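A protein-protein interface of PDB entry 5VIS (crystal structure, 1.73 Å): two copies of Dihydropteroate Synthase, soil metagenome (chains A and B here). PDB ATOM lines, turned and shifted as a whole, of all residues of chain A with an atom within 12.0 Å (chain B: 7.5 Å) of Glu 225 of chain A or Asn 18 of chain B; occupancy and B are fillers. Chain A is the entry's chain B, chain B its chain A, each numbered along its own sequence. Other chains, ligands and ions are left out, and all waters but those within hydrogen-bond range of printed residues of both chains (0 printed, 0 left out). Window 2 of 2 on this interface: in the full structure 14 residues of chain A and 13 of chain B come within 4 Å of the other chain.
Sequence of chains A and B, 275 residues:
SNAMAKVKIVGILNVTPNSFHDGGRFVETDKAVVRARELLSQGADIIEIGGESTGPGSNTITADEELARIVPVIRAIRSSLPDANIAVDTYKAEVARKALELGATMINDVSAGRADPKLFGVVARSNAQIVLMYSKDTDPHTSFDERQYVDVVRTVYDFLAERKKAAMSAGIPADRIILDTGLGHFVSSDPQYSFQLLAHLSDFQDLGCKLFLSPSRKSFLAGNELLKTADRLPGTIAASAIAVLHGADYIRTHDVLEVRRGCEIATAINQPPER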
ATOM      1  N   PRO A 191       6.907 -22.111  17.829  1.00  0.00           N
ATOM      2  CA  PRO A 191       5.990 -20.957  17.934  1.00  0.00           C
ATOM      3  C   PRO A 191       6.591 -19.582  18.241  1.00  0.00           C
ATOM      4  O   PRO A 191       5.973 -18.578  17.907  1.00  0.00           O
ATOM      5  CB  PRO A 191       5.030 -21.351  19.095  1.00  0.00           C
ATOM      6  CG  PRO A 191       5.647 -22.487  19.760  1.00  0.00           C
ATOM      7  CD  PRO A 191       6.700 -23.097  18.908  1.00  0.00           C
ATOM      8  N   PHE A 195       5.213 -15.252  17.406  1.00  0.00           N
ATOM      9  CA  PHE A 195       5.005 -14.209  18.393  1.00  0.00           C
ATOM     10  C   PHE A 195       5.919 -13.002  18.141  1.00  0.00           C
ATOM     11  O   PHE A 195       5.491 -11.877  18.329  1.00  0.00           O
ATOM     12  CB  PHE A 195       5.196 -14.746  19.796  1.00  0.00           C
ATOM     13  CG  PHE A 195       4.167 -15.788  20.176  1.00  0.00           C
ATOM     14  CD1 PHE A 195       2.818 -15.480  20.167  1.00  0.00           C
ATOM     15  CD2 PHE A 195       4.560 -17.066  20.587  1.00  0.00           C
ATOM     16  CE1 PHE A 195       1.854 -16.430  20.529  1.00  0.00           C
ATOM     17  CE2 PHE A 195       3.616 -17.996  20.965  1.00  0.00           C
ATOM     18  CZ  PHE A 195       2.278 -17.695  20.933  1.00  0.00           C
ATOM     19  N   LYS A 218      -4.122 -21.389  14.657  1.00  0.00           N
ATOM     20  CA  LYS A 218      -2.899 -22.122  14.317  1.00  0.00           C
ATOM     21  C   LYS A 218      -2.246 -22.674  15.581  1.00  0.00           C
ATOM     22  O   LYS A 218      -2.429 -22.151  16.679  1.00  0.00           O
ATOM     23  CB  LYS A 218      -1.926 -21.230  13.542  1.00  0.00           C
ATOM     24  CG  LYS A 218      -2.352 -20.929  12.119  1.00  0.00           C
ATOM     25  CD  LYS A 218      -1.362 -19.979  11.450  1.00  0.00           C
ATOM     26  CE  LYS A 218      -1.526 -19.978   9.935  1.00  0.00           C
ATOM     27  NZ  LYS A 218      -2.825 -19.470   9.467  1.00  0.00           N
ATOM     28  N   SER A 219      -1.488 -23.743  15.417  1.00  0.00           N
ATOM     29  CA  SER A 219      -0.846 -24.403  16.564  1.00  0.00           C
ATOM     30  C   SER A 219       0.167 -23.571  17.345  1.00  0.00           C
ATOM     31  O   SER A 219       0.464 -23.922  18.495  1.00  0.00           O
ATOM     32  CB  SER A 219      -0.259 -25.744  16.160  1.00  0.00           C
ATOM     33  OG  SER A 219       0.720 -25.584  15.173  1.00  0.00           O
ATOM     34  N   PHE A 220       0.651 -22.455  16.787  1.00  0.00           N
ATOM     35  CA  PHE A 220       1.566 -21.586  17.565  1.00  0.00           C
ATOM     36  C   PHE A 220       0.834 -21.013  18.790  1.00  0.00           C
ATOM     37  O   PHE A 220       1.473 -20.561  19.744  1.00  0.00           O
ATOM     38  CB  PHE A 220       2.230 -20.457  16.743  1.00  0.00           C
ATOM     39  CG  PHE A 220       1.358 -19.274  16.444  1.00  0.00           C
ATOM     40  CD1 PHE A 220       0.529 -19.269  15.340  1.00  0.00           C
ATOM     41  CD2 PHE A 220       1.403 -18.132  17.257  1.00  0.00           C
ATOM     42  CE1 PHE A 220      -0.265 -18.167  15.060  1.00  0.00           C
ATOM     43  CE2 PHE A 220       0.612 -17.025  16.966  1.00  0.00           C
ATOM     44  CZ  PHE A 220      -0.220 -17.056  15.872  1.00  0.00           C
ATOM     45  N   LEU A 221      -0.498 -21.085  18.750  1.00  0.00           N
ATOM     46  CA  LEU A 221      -1.342 -20.613  19.832  1.00  0.00           C
ATOM     47  C   LEU A 221      -1.638 -21.699  20.867  1.00  0.00           C
ATOM     48  O   LEU A 221      -2.407 -21.460  21.792  1.00  0.00           O
ATOM     49  CB  LEU A 221      -2.658 -20.064  19.254  1.00  0.00           C
ATOM     50  CG  LEU A 221      -2.506 -18.853  18.329  1.00  0.00           C
ATOM     51  CD1 LEU A 221      -3.784 -18.592  17.562  1.00  0.00           C
ATOM     52  CD2 LEU A 221      -2.097 -17.599  19.077  1.00  0.00           C
ATOM     53  N   ALA A 222      -1.012 -22.869  20.747  1.00  0.00           N
ATOM     54  CA  ALA A 222      -1.275 -23.971  21.705  1.00  0.00           C
ATOM     55  C   ALA A 222      -0.856 -23.635  23.137  1.00  0.00           C
ATOM     56  O   ALA A 222      -1.499 -24.086  24.096  1.00  0.00           O
ATOM     57  CB  ALA A 222      -0.605 -25.253  21.245  1.00  0.00           C
ATOM     58  N   GLY A 223       0.202 -22.836  23.290  1.00  0.00           N
ATOM     59  CA  GLY A 223       0.670 -22.435  24.630  1.00  0.00           C
ATOM     60  C   GLY A 223       1.166 -23.562  25.519  1.00  0.00           C
ATOM     61  O   GLY A 223       1.353 -24.696  25.078  1.00  0.00           O
ATOM     62  N   ASN A 224       1.353 -23.241  26.802  1.00  0.00           N
ATOM     63  CA  ASN A 224       1.839 -24.213  27.790  1.00  0.00           C
ATOM     64  C   ASN A 224       0.890 -25.388  28.009  1.00  0.00           C
ATOM     65  O   ASN A 224       1.329 -26.484  28.367  1.00  0.00           O
ATOM     66  CB  ASN A 224       2.117 -23.528  29.150  1.00  0.00           C
ATOM     67  CG  ASN A 224       3.328 -22.597  29.121  1.00  0.00           C
ATOM     68  OD1 ASN A 224       4.089 -22.553  28.149  1.00  0.00           O
ATOM     69  ND2 ASN A 224       3.528 -21.867  30.222  1.00  0.00           N
ATOM     70  N   GLU A 225      -0.408 -25.158  27.830  1.00  0.00           N
ATOM     71  CA  GLU A 225      -1.407 -26.220  27.997  1.00  0.00           C
ATOM     72  C   GLU A 225      -1.543 -27.154  26.784  1.00  0.00           C
ATOM     73  O   GLU A 225      -2.296 -28.126  26.855  1.00  0.00           O
ATOM     74  CB  GLU A 225      -2.777 -25.610  28.289  1.00  0.00           C
ATOM     75  CG  GLU A 225      -2.911 -24.957  29.654  1.00  0.00           C
ATOM     76  CD  GLU A 225      -4.224 -24.215  29.787  1.00  0.00           C
ATOM     77  OE1 GLU A 225      -4.351 -23.081  29.255  1.00  0.00           O
ATOM     78  OE2 GLU A 225      -5.117 -24.738  30.471  1.00  0.00           O
ATOM     79  N   LEU A 226      -0.821 -26.865  25.703  1.00  0.00           N
ATOM     80  CA  LEU A 226      -0.901 -27.678  24.451  1.00  0.00           C
ATOM     81  C   LEU A 226      -2.367 -27.773  23.979  1.00  0.00           C
ATOM     82  O   LEU A 226      -2.925 -28.840  23.700  1.00  0.00           O
ATOM     83  CB  LEU A 226      -0.265 -29.056  24.640  1.00  0.00           C
ATOM     84  CG  LEU A 226       1.204 -29.042  25.095  1.00  0.00           C
ATOM     85  CD1 LEU A 226       1.724 -30.469  25.168  1.00  0.00           C
ATOM     86  CD2 LEU A 226       2.100 -28.213  24.187  1.00  0.00           C
ATOM     87  N   LEU A 227      -2.984 -26.615  23.901  1.00  0.00           N
ATOM     88  CA  LEU A 227      -4.369 -26.510  23.527  1.00  0.00           C
ATOM     89  C   LEU A 227      -4.627 -26.955  22.105  1.00  0.00           C
ATOM     90  O   LEU A 227      -3.869 -26.587  21.180  1.00  0.00           O
ATOM     91  CB  LEU A 227      -4.834 -25.063  23.647  1.00  0.00           C
ATOM     92  CG  LEU A 227      -4.757 -24.411  25.033  1.00  0.00           C
ATOM     93  CD1 LEU A 227      -5.048 -22.918  24.919  1.00  0.00           C
ATOM     94  CD2 LEU A 227      -5.708 -25.116  25.996  1.00  0.00           C
ATOM     95  N   LYS A 228      -5.693 -27.734  21.928  1.00  0.00           N
ATOM     96  CA  LYS A 228      -6.086 -28.198  20.608  1.00  0.00           C
ATOM     97  C   LYS A 228      -6.940 -27.114  19.962  1.00  0.00           C
ATOM     98  O   LYS A 228      -7.340 -26.161  20.629  1.00  0.00           O
ATOM     99  CB  LYS A 228      -6.853 -29.502  20.709  1.00  0.00           C
ATOM    100  CG  LYS A 228      -6.118 -30.550  21.529  1.00  0.00           C
ATOM    101  CD  LYS A 228      -4.625 -30.562  21.211  1.00  0.00           C
ATOM    102  CE  LYS A 228      -4.355 -30.564  19.720  1.00  0.00           C
ATOM    103  NZ  LYS A 228      -2.919 -30.790  19.414  1.00  0.00           N
ATOM    104  N   THR A 229      -7.236 -27.279  18.673  1.00  0.00           N
ATOM    105  CA  THR A 229      -8.021 -26.286  17.904  1.00  0.00           C
ATOM    106  C   THR A 229      -9.265 -25.719  18.575  1.00  0.00           C
ATOM    107  O   THR A 229      -9.460 -24.502  18.603  1.00  0.00           O
ATOM    108  CB  THR A 229      -8.427 -26.881  16.546  1.00  0.00           C
ATOM    109  OG1 THR A 229      -7.235 -27.198  15.826  1.00  0.00           O
ATOM    110  CG2 THR A 229      -9.288 -25.890  15.727  1.00  0.00           C
ATOM    111  N   ALA A 230     -10.073 -26.601  19.153  1.00  0.00           N
ATOM    112  CA  ALA A 230     -11.321 -26.181  19.800  1.00  0.00           C
ATOM    113  C   ALA A 230     -11.123 -25.164  20.906  1.00  0.00           C
ATOM    114  O   ALA A 230     -12.023 -24.373  21.170  1.00  0.00           O
ATOM    115  CB  ALA A 230     -12.080 -27.393  20.346  1.00  0.00           C
ATOM    116  N   ASP A 231      -9.952 -25.186  21.531  1.00  0.00           N
ATOM    117  CA  ASP A 231      -9.639 -24.309  22.670  1.00  0.00           C
ATOM    118  C   ASP A 231      -8.763 -23.092  22.342  1.00  0.00           C
ATOM    119  O   ASP A 231      -8.377 -22.357  23.251  1.00  0.00           O
ATOM    120  CB  ASP A 231      -8.946 -25.132  23.773  1.00  0.00           C
ATOM    121  CG  ASP A 231      -9.860 -26.187  24.400  1.00  0.00           C
ATOM    122  OD1 ASP A 231     -11.089 -25.966  24.492  1.00  0.00           O
ATOM    123  OD2 ASP A 231      -9.317 -27.222  24.853  1.00  0.00           O
ATOM    124  N   ARG A 232      -8.492 -22.857  21.058  1.00  0.00           N
ATOM    125  CA  ARG A 232      -7.633 -21.737  20.657  1.00  0.00           C
ATOM    126  C   ARG A 232      -8.358 -20.445  20.294  1.00  0.00           C
ATOM    127  O   ARG A 232      -7.712 -19.528  19.766  1.00  0.00           O
ATOM    128  CB  ARG A 232      -6.746 -22.174  19.476  1.00  0.00           C
ATOM    129  CG  ARG A 232      -5.752 -23.267  19.845  1.00  0.00           C
ATOM    130  CD  ARG A 232      -5.029 -23.741  18.598  1.00  0.00           C
ATOM    131  NE  ARG A 232      -4.307 -24.968  18.863  1.00  0.00           N
ATOM    132  CZ  ARG A 232      -3.871 -25.809  17.933  1.00  0.00           C
ATOM    133  NH1 ARG A 232      -4.091 -25.585  16.627  1.00  0.00           N
ATOM    134  NH2 ARG A 232      -3.241 -26.914  18.321  1.00  0.00           N
ATOM    135  N   LEU A 233      -9.663 -20.339  20.571  1.00  0.00           N
ATOM    136  CA  LEU A 233     -10.367 -19.095  20.206  1.00  0.00           C
ATOM    137  C   LEU A 233      -9.858 -17.880  21.002  1.00  0.00           C
ATOM    138  O   LEU A 233      -9.588 -16.840  20.409  1.00  0.00           O
ATOM    139  CB  LEU A 233     -11.885 -19.239  20.270  1.00  0.00           C
ATOM    140  CG  LEU A 233     -12.656 -17.995  19.808  1.00  0.00           C
ATOM    141  CD1 LEU A 233     -12.208 -17.530  18.423  1.00  0.00           C
ATOM    142  CD2 LEU A 233     -14.155 -18.251  19.844  1.00  0.00           C
ATOM    143  N   PRO A 234      -9.724 -18.003  22.345  1.00  0.00           N
ATOM    144  CA  PRO A 234      -9.201 -16.838  23.072  1.00  0.00           C
ATOM    145  C   PRO A 234      -7.843 -16.376  22.555  1.00  0.00           C
ATOM    146  O   PRO A 234      -7.624 -15.164  22.366  1.00  0.00           O
ATOM    147  CB  PRO A 234      -9.143 -17.329  24.521  1.00  0.00           C
ATOM    148  CG  PRO A 234     -10.234 -18.342  24.598  1.00  0.00           C
ATOM    149  CD  PRO A 234     -10.159 -19.057  23.271  1.00  0.00           C
ATOM    150  N   GLY A 235      -6.958 -17.329  22.270  1.00  0.00           N
ATOM    151  CA  GLY A 235      -5.620 -16.975  21.754  1.00  0.00           C
ATOM    152  C   GLY A 235      -5.705 -16.323  20.386  1.00  0.00           C
ATOM    153  O   GLY A 235      -4.929 -15.425  20.077  1.00  0.00           O
ATOM    154  N   THR A 236      -6.628 -16.812  19.555  1.00  0.00           N
ATOM    155  CA  THR A 236      -6.830 -16.256  18.212  1.00  0.00           C
ATOM    156  C   THR A 236      -7.344 -14.826  18.300  1.00  0.00           C
ATOM    157  O   THR A 236      -6.940 -13.950  17.523  1.00  0.00           O
ATOM    158  CB  THR A 236      -7.806 -17.136  17.401  1.00  0.00           C
ATOM    159  OG1 THR A 236      -7.233 -18.444  17.274  1.00  0.00           O
ATOM    160  CG2 THR A 236      -8.040 -16.584  16.033  1.00  0.00           C
ATOM    161  N   THR B  16      -0.671 -30.994  34.573  1.00  0.00           N
ATOM    162  CA  THR B  16      -0.157 -29.696  34.100  1.00  0.00           C
ATOM    163  C   THR B  16      -0.943 -28.593  34.781  1.00  0.00           C
ATOM    164  O   THR B  16      -2.158 -28.519  34.607  1.00  0.00           O
ATOM    165  CB  THR B  16      -0.312 -29.541  32.573  1.00  0.00           C
ATOM    166  OG1 THR B  16       0.519 -30.506  31.906  1.00  0.00           O
ATOM    167  CG2 THR B  16       0.097 -28.129  32.106  1.00  0.00           C
ATOM    168  N   PRO B  17      -0.268 -27.735  35.565  1.00  0.00           N
ATOM    169  CA  PRO B  17      -1.012 -26.652  36.225  1.00  0.00           C
ATOM    170  C   PRO B  17      -1.568 -25.631  35.230  1.00  0.00           C
ATOM    171  O   PRO B  17      -1.000 -25.462  34.145  1.00  0.00           O
ATOM    172  CB  PRO B  17       0.043 -25.982  37.125  1.00  0.00           C
ATOM    173  CG  PRO B  17       1.162 -26.956  37.239  1.00  0.00           C
ATOM    174  CD  PRO B  17       1.149 -27.766  35.973  1.00  0.00           C
ATOM    175  N   ASN B  18      -2.687 -24.996  35.581  1.00  0.00           N
ATOM    176  CA  ASN B  18      -3.285 -23.938  34.742  1.00  0.00           C
ATOM    177  C   ASN B  18      -2.568 -22.652  35.068  1.00  0.00           C
ATOM    178  O   ASN B  18      -2.056 -21.965  34.180  1.00  0.00           O
ATOM    179  CB  ASN B  18      -4.797 -23.760  34.980  1.00  0.00           C
ATOM    180  CG  ASN B  18      -5.647 -24.768  34.218  1.00  0.00           C
ATOM    181  OD1 ASN B  18      -5.147 -25.762  33.676  1.00  0.00           O
ATOM    182  ND2 ASN B  18      -6.953 -24.497  34.159  1.00  0.00           N
ATOM    183  N   SER B  19      -2.537 -22.339  36.359  1.00  0.00           N
ATOM    184  CA  SER B  19      -1.874 -21.145  36.844  1.00  0.00           C
ATOM    185  C   SER B  19      -0.351 -21.304  36.736  1.00  0.00           C
ATOM    186  O   SER B  19       0.223 -22.273  37.246  1.00  0.00           O
ATOM    187  CB  SER B  19      -2.293 -20.861  38.287  1.00  0.00           C
ATOM    188  OG  SER B  19      -1.588 -19.754  38.809  1.00  0.00           O
ATOM    189  N   PHE B  20       0.280 -20.343  36.060  1.00  0.00           N
ATOM    190  CA  PHE B  20       1.734 -20.323  35.856  1.00  0.00           C
ATOM    191  C   PHE B  20       2.483 -20.009  37.165  1.00  0.00           C
ATOM    192  O   PHE B  20       3.611 -20.469  37.369  1.00  0.00           O
ATOM    193  CB  PHE B  20       2.072 -19.285  34.761  1.00  0.00           C
ATOM    194  CG  PHE B  20       3.537 -19.223  34.373  1.00  0.00           C
ATOM    195  CD1 PHE B  20       4.064 -20.109  33.429  1.00  0.00           C
ATOM    196  CD2 PHE B  20       4.380 -18.245  34.913  1.00  0.00           C
ATOM    197  CE1 PHE B  20       5.404 -20.043  33.058  1.00  0.00           C
ATOM    198  CE2 PHE B  20       5.720 -18.174  34.541  1.00  0.00           C
ATOM    199  CZ  PHE B  20       6.233 -19.075  33.613  1.00  0.00           C
ATOM    200  N   HIS B  21       1.836 -19.246  38.049  1.00  0.00           N
ATOM    201  CA  HIS B  21       2.416 -18.838  39.334  1.00  0.00           C
ATOM    202  C   HIS B  21       2.139 -19.878  40.434  1.00  0.00           C
ATOM    203  O   HIS B  21       1.509 -20.903  40.181  1.00  0.00           O
ATOM    204  CB  HIS B  21       1.827 -17.480  39.729  1.00  0.00           C
ATOM    205  CG  HIS B  21       1.916 -16.453  38.641  1.00  0.00           C
ATOM    206  ND1 HIS B  21       2.971 -15.575  38.529  1.00  0.00           N
ATOM    207  CD2 HIS B  21       1.091 -16.187  37.598  1.00  0.00           C
ATOM    208  CE1 HIS B  21       2.788 -14.804  37.471  1.00  0.00           C
ATOM    209  NE2 HIS B  21       1.656 -15.157  36.887  1.00  0.00           N
ATOM    210  N   GLY B  23       0.517 -21.502  43.937  1.00  0.00           N
ATOM    211  CA  GLY B  23      -0.828 -21.569  44.516  1.00  0.00           C
ATOM    212  C   GLY B  23      -1.727 -22.402  43.619  1.00  0.00           C
ATOM    213  O   GLY B  23      -1.410 -22.611  42.444  1.00  0.00           O
ATOM    214  N   GLY B  24      -2.843 -22.882  44.169  1.00  0.00           N
ATOM    215  CA  GLY B  24      -3.801 -23.693  43.402  1.00  0.00           C
ATOM    216  C   GLY B  24      -3.339 -25.110  43.070  1.00  0.00           C
ATOM    217  O   GLY B  24      -3.825 -25.711  42.103  1.00  0.00           O
ATOM    218  N   GLU B  28      -5.546 -28.690  41.490  1.00  0.00           N
ATOM    219  CA  GLU B  28      -5.018 -29.446  40.342  1.00  0.00           C
ATOM    220  C   GLU B  28      -4.836 -30.935  40.723  1.00  0.00           C
ATOM    221  O   GLU B  28      -5.115 -31.840  39.926  1.00  0.00           O
ATOM    222  CB  GLU B  28      -3.694 -28.840  39.863  1.00  0.00           C
ATOM    223  CG  GLU B  28      -2.978 -29.593  38.738  1.00  0.00           C
ATOM    224  CD  GLU B  28      -3.772 -29.702  37.434  1.00  0.00           C
ATOM    225  OE1 GLU B  28      -4.643 -28.834  37.162  1.00  0.00           O
ATOM    226  OE2 GLU B  28      -3.498 -30.657  36.663  1.00  0.00           O
ATOM    227  N   LYS B  31      -8.235 -32.526  40.752  1.00  0.00           N
ATOM    228  CA  LYS B  31      -8.701 -32.753  39.368  1.00  0.00           C
ATOM    229  C   LYS B  31      -8.064 -34.002  38.761  1.00  0.00           C
ATOM    230  O   LYS B  31      -8.734 -34.773  38.045  1.00  0.00           O
ATOM    231  CB  LYS B  31      -8.406 -31.534  38.485  1.00  0.00           C
ATOM    232  CG  LYS B  31      -9.288 -30.339  38.796  1.00  0.00           C
ATOM    233  CD  LYS B  31      -8.763 -29.033  38.187  1.00  0.00           C
ATOM    234  CE  LYS B  31      -8.697 -29.029  36.670  1.00  0.00           C
ATOM    235  NZ  LYS B  31      -8.272 -27.664  36.211  1.00  0.00           N
ATOM    236  N   SER B  53       5.423 -32.963  29.653  1.00  0.00           N
ATOM    237  CA  SER B  53       5.073 -33.373  28.296  1.00  0.00           C
ATOM    238  C   SER B  53       6.357 -33.466  27.470  1.00  0.00           C
ATOM    239  O   SER B  53       7.253 -32.649  27.649  1.00  0.00           O
ATOM    240  CB  SER B  53       4.142 -32.339  27.668  1.00  0.00           C
ATOM    241  OG  SER B  53       2.956 -32.239  28.432  1.00  0.00           O
ATOM    242  N   ASN B  59       7.678 -27.966  26.809  1.00  0.00           N
ATOM    243  CA  ASN B  59       8.695 -27.295  27.609  1.00  0.00           C
ATOM    244  C   ASN B  59       9.366 -28.261  28.587  1.00  0.00           C
ATOM    245  O   ASN B  59       8.740 -29.182  29.107  1.00  0.00           O
ATOM    246  CB  ASN B  59       8.063 -26.148  28.417  1.00  0.00           C
ATOM    247  CG  ASN B  59       7.494 -25.043  27.542  1.00  0.00           C
ATOM    248  OD1 ASN B  59       7.951 -24.807  26.416  1.00  0.00           O
ATOM    249  ND2 ASN B  59       6.504 -24.333  28.073  1.00  0.00           N
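ND2 of Asn 59 of chain B is in hydrogen-bond range of OD1 of Asn 224 of chain A. The side-chain carboxylate (OE2) of Glu 225 of chain A sits close to the side-chain amide oxygen (OD1) of Asn 18 of chain B (3.4 Å).
Of chain B, only Asn 18 (3.4 Å) comes within 4 Å of Glu 225 of chain A. Of chain A, only Glu 225 comes within 4 Å of Asn 18 of chain B. No residue of chain A comes within 4 Å of Thr 16 of chain B. No residue of chain A comes within 4 Å of Pro 17 of chain B. Of the printed residues of chain A, Phe 20 of chain B touches Asn 224. Of the printed residues of chain A, Ser 53 of chain B touches Leu 226 (3.9 Å). Leu 233 of chain A touches none of the printed residues of chain B. Thr 229 of chain A touches none of the printed residues of chain B. The nearest residue of chain A that does not touch Asn 18 of chain B is Asn 224 of chain A (6.7 Å).
Among the printed residues, pairs that only touch across the chains: Asn 224 of chain A with Phe 20 of chain B and Leu 226 of chain A with Ser 53 of chain B.
No position is printed for both chains. Of the 4 pairs that touch across the chains among the printed residues, none has its exchanged pair printed and touching as well.
Of the 21 printed residues of chain A, 3 touch a printed residue of chain B. Printed residues of chain A that touch a printed residue of chain B: Asn 224, Glu 225 and Leu 226. Hydrophobic or aromatic side chains of chain A that line the printed part of chain B: Leu 226. Hydrophobic or aromatic side chains of chain B within 4 Å of the printed part of chain A: Phe 20. Among the printed residues, 4 pairs touch across the chains.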
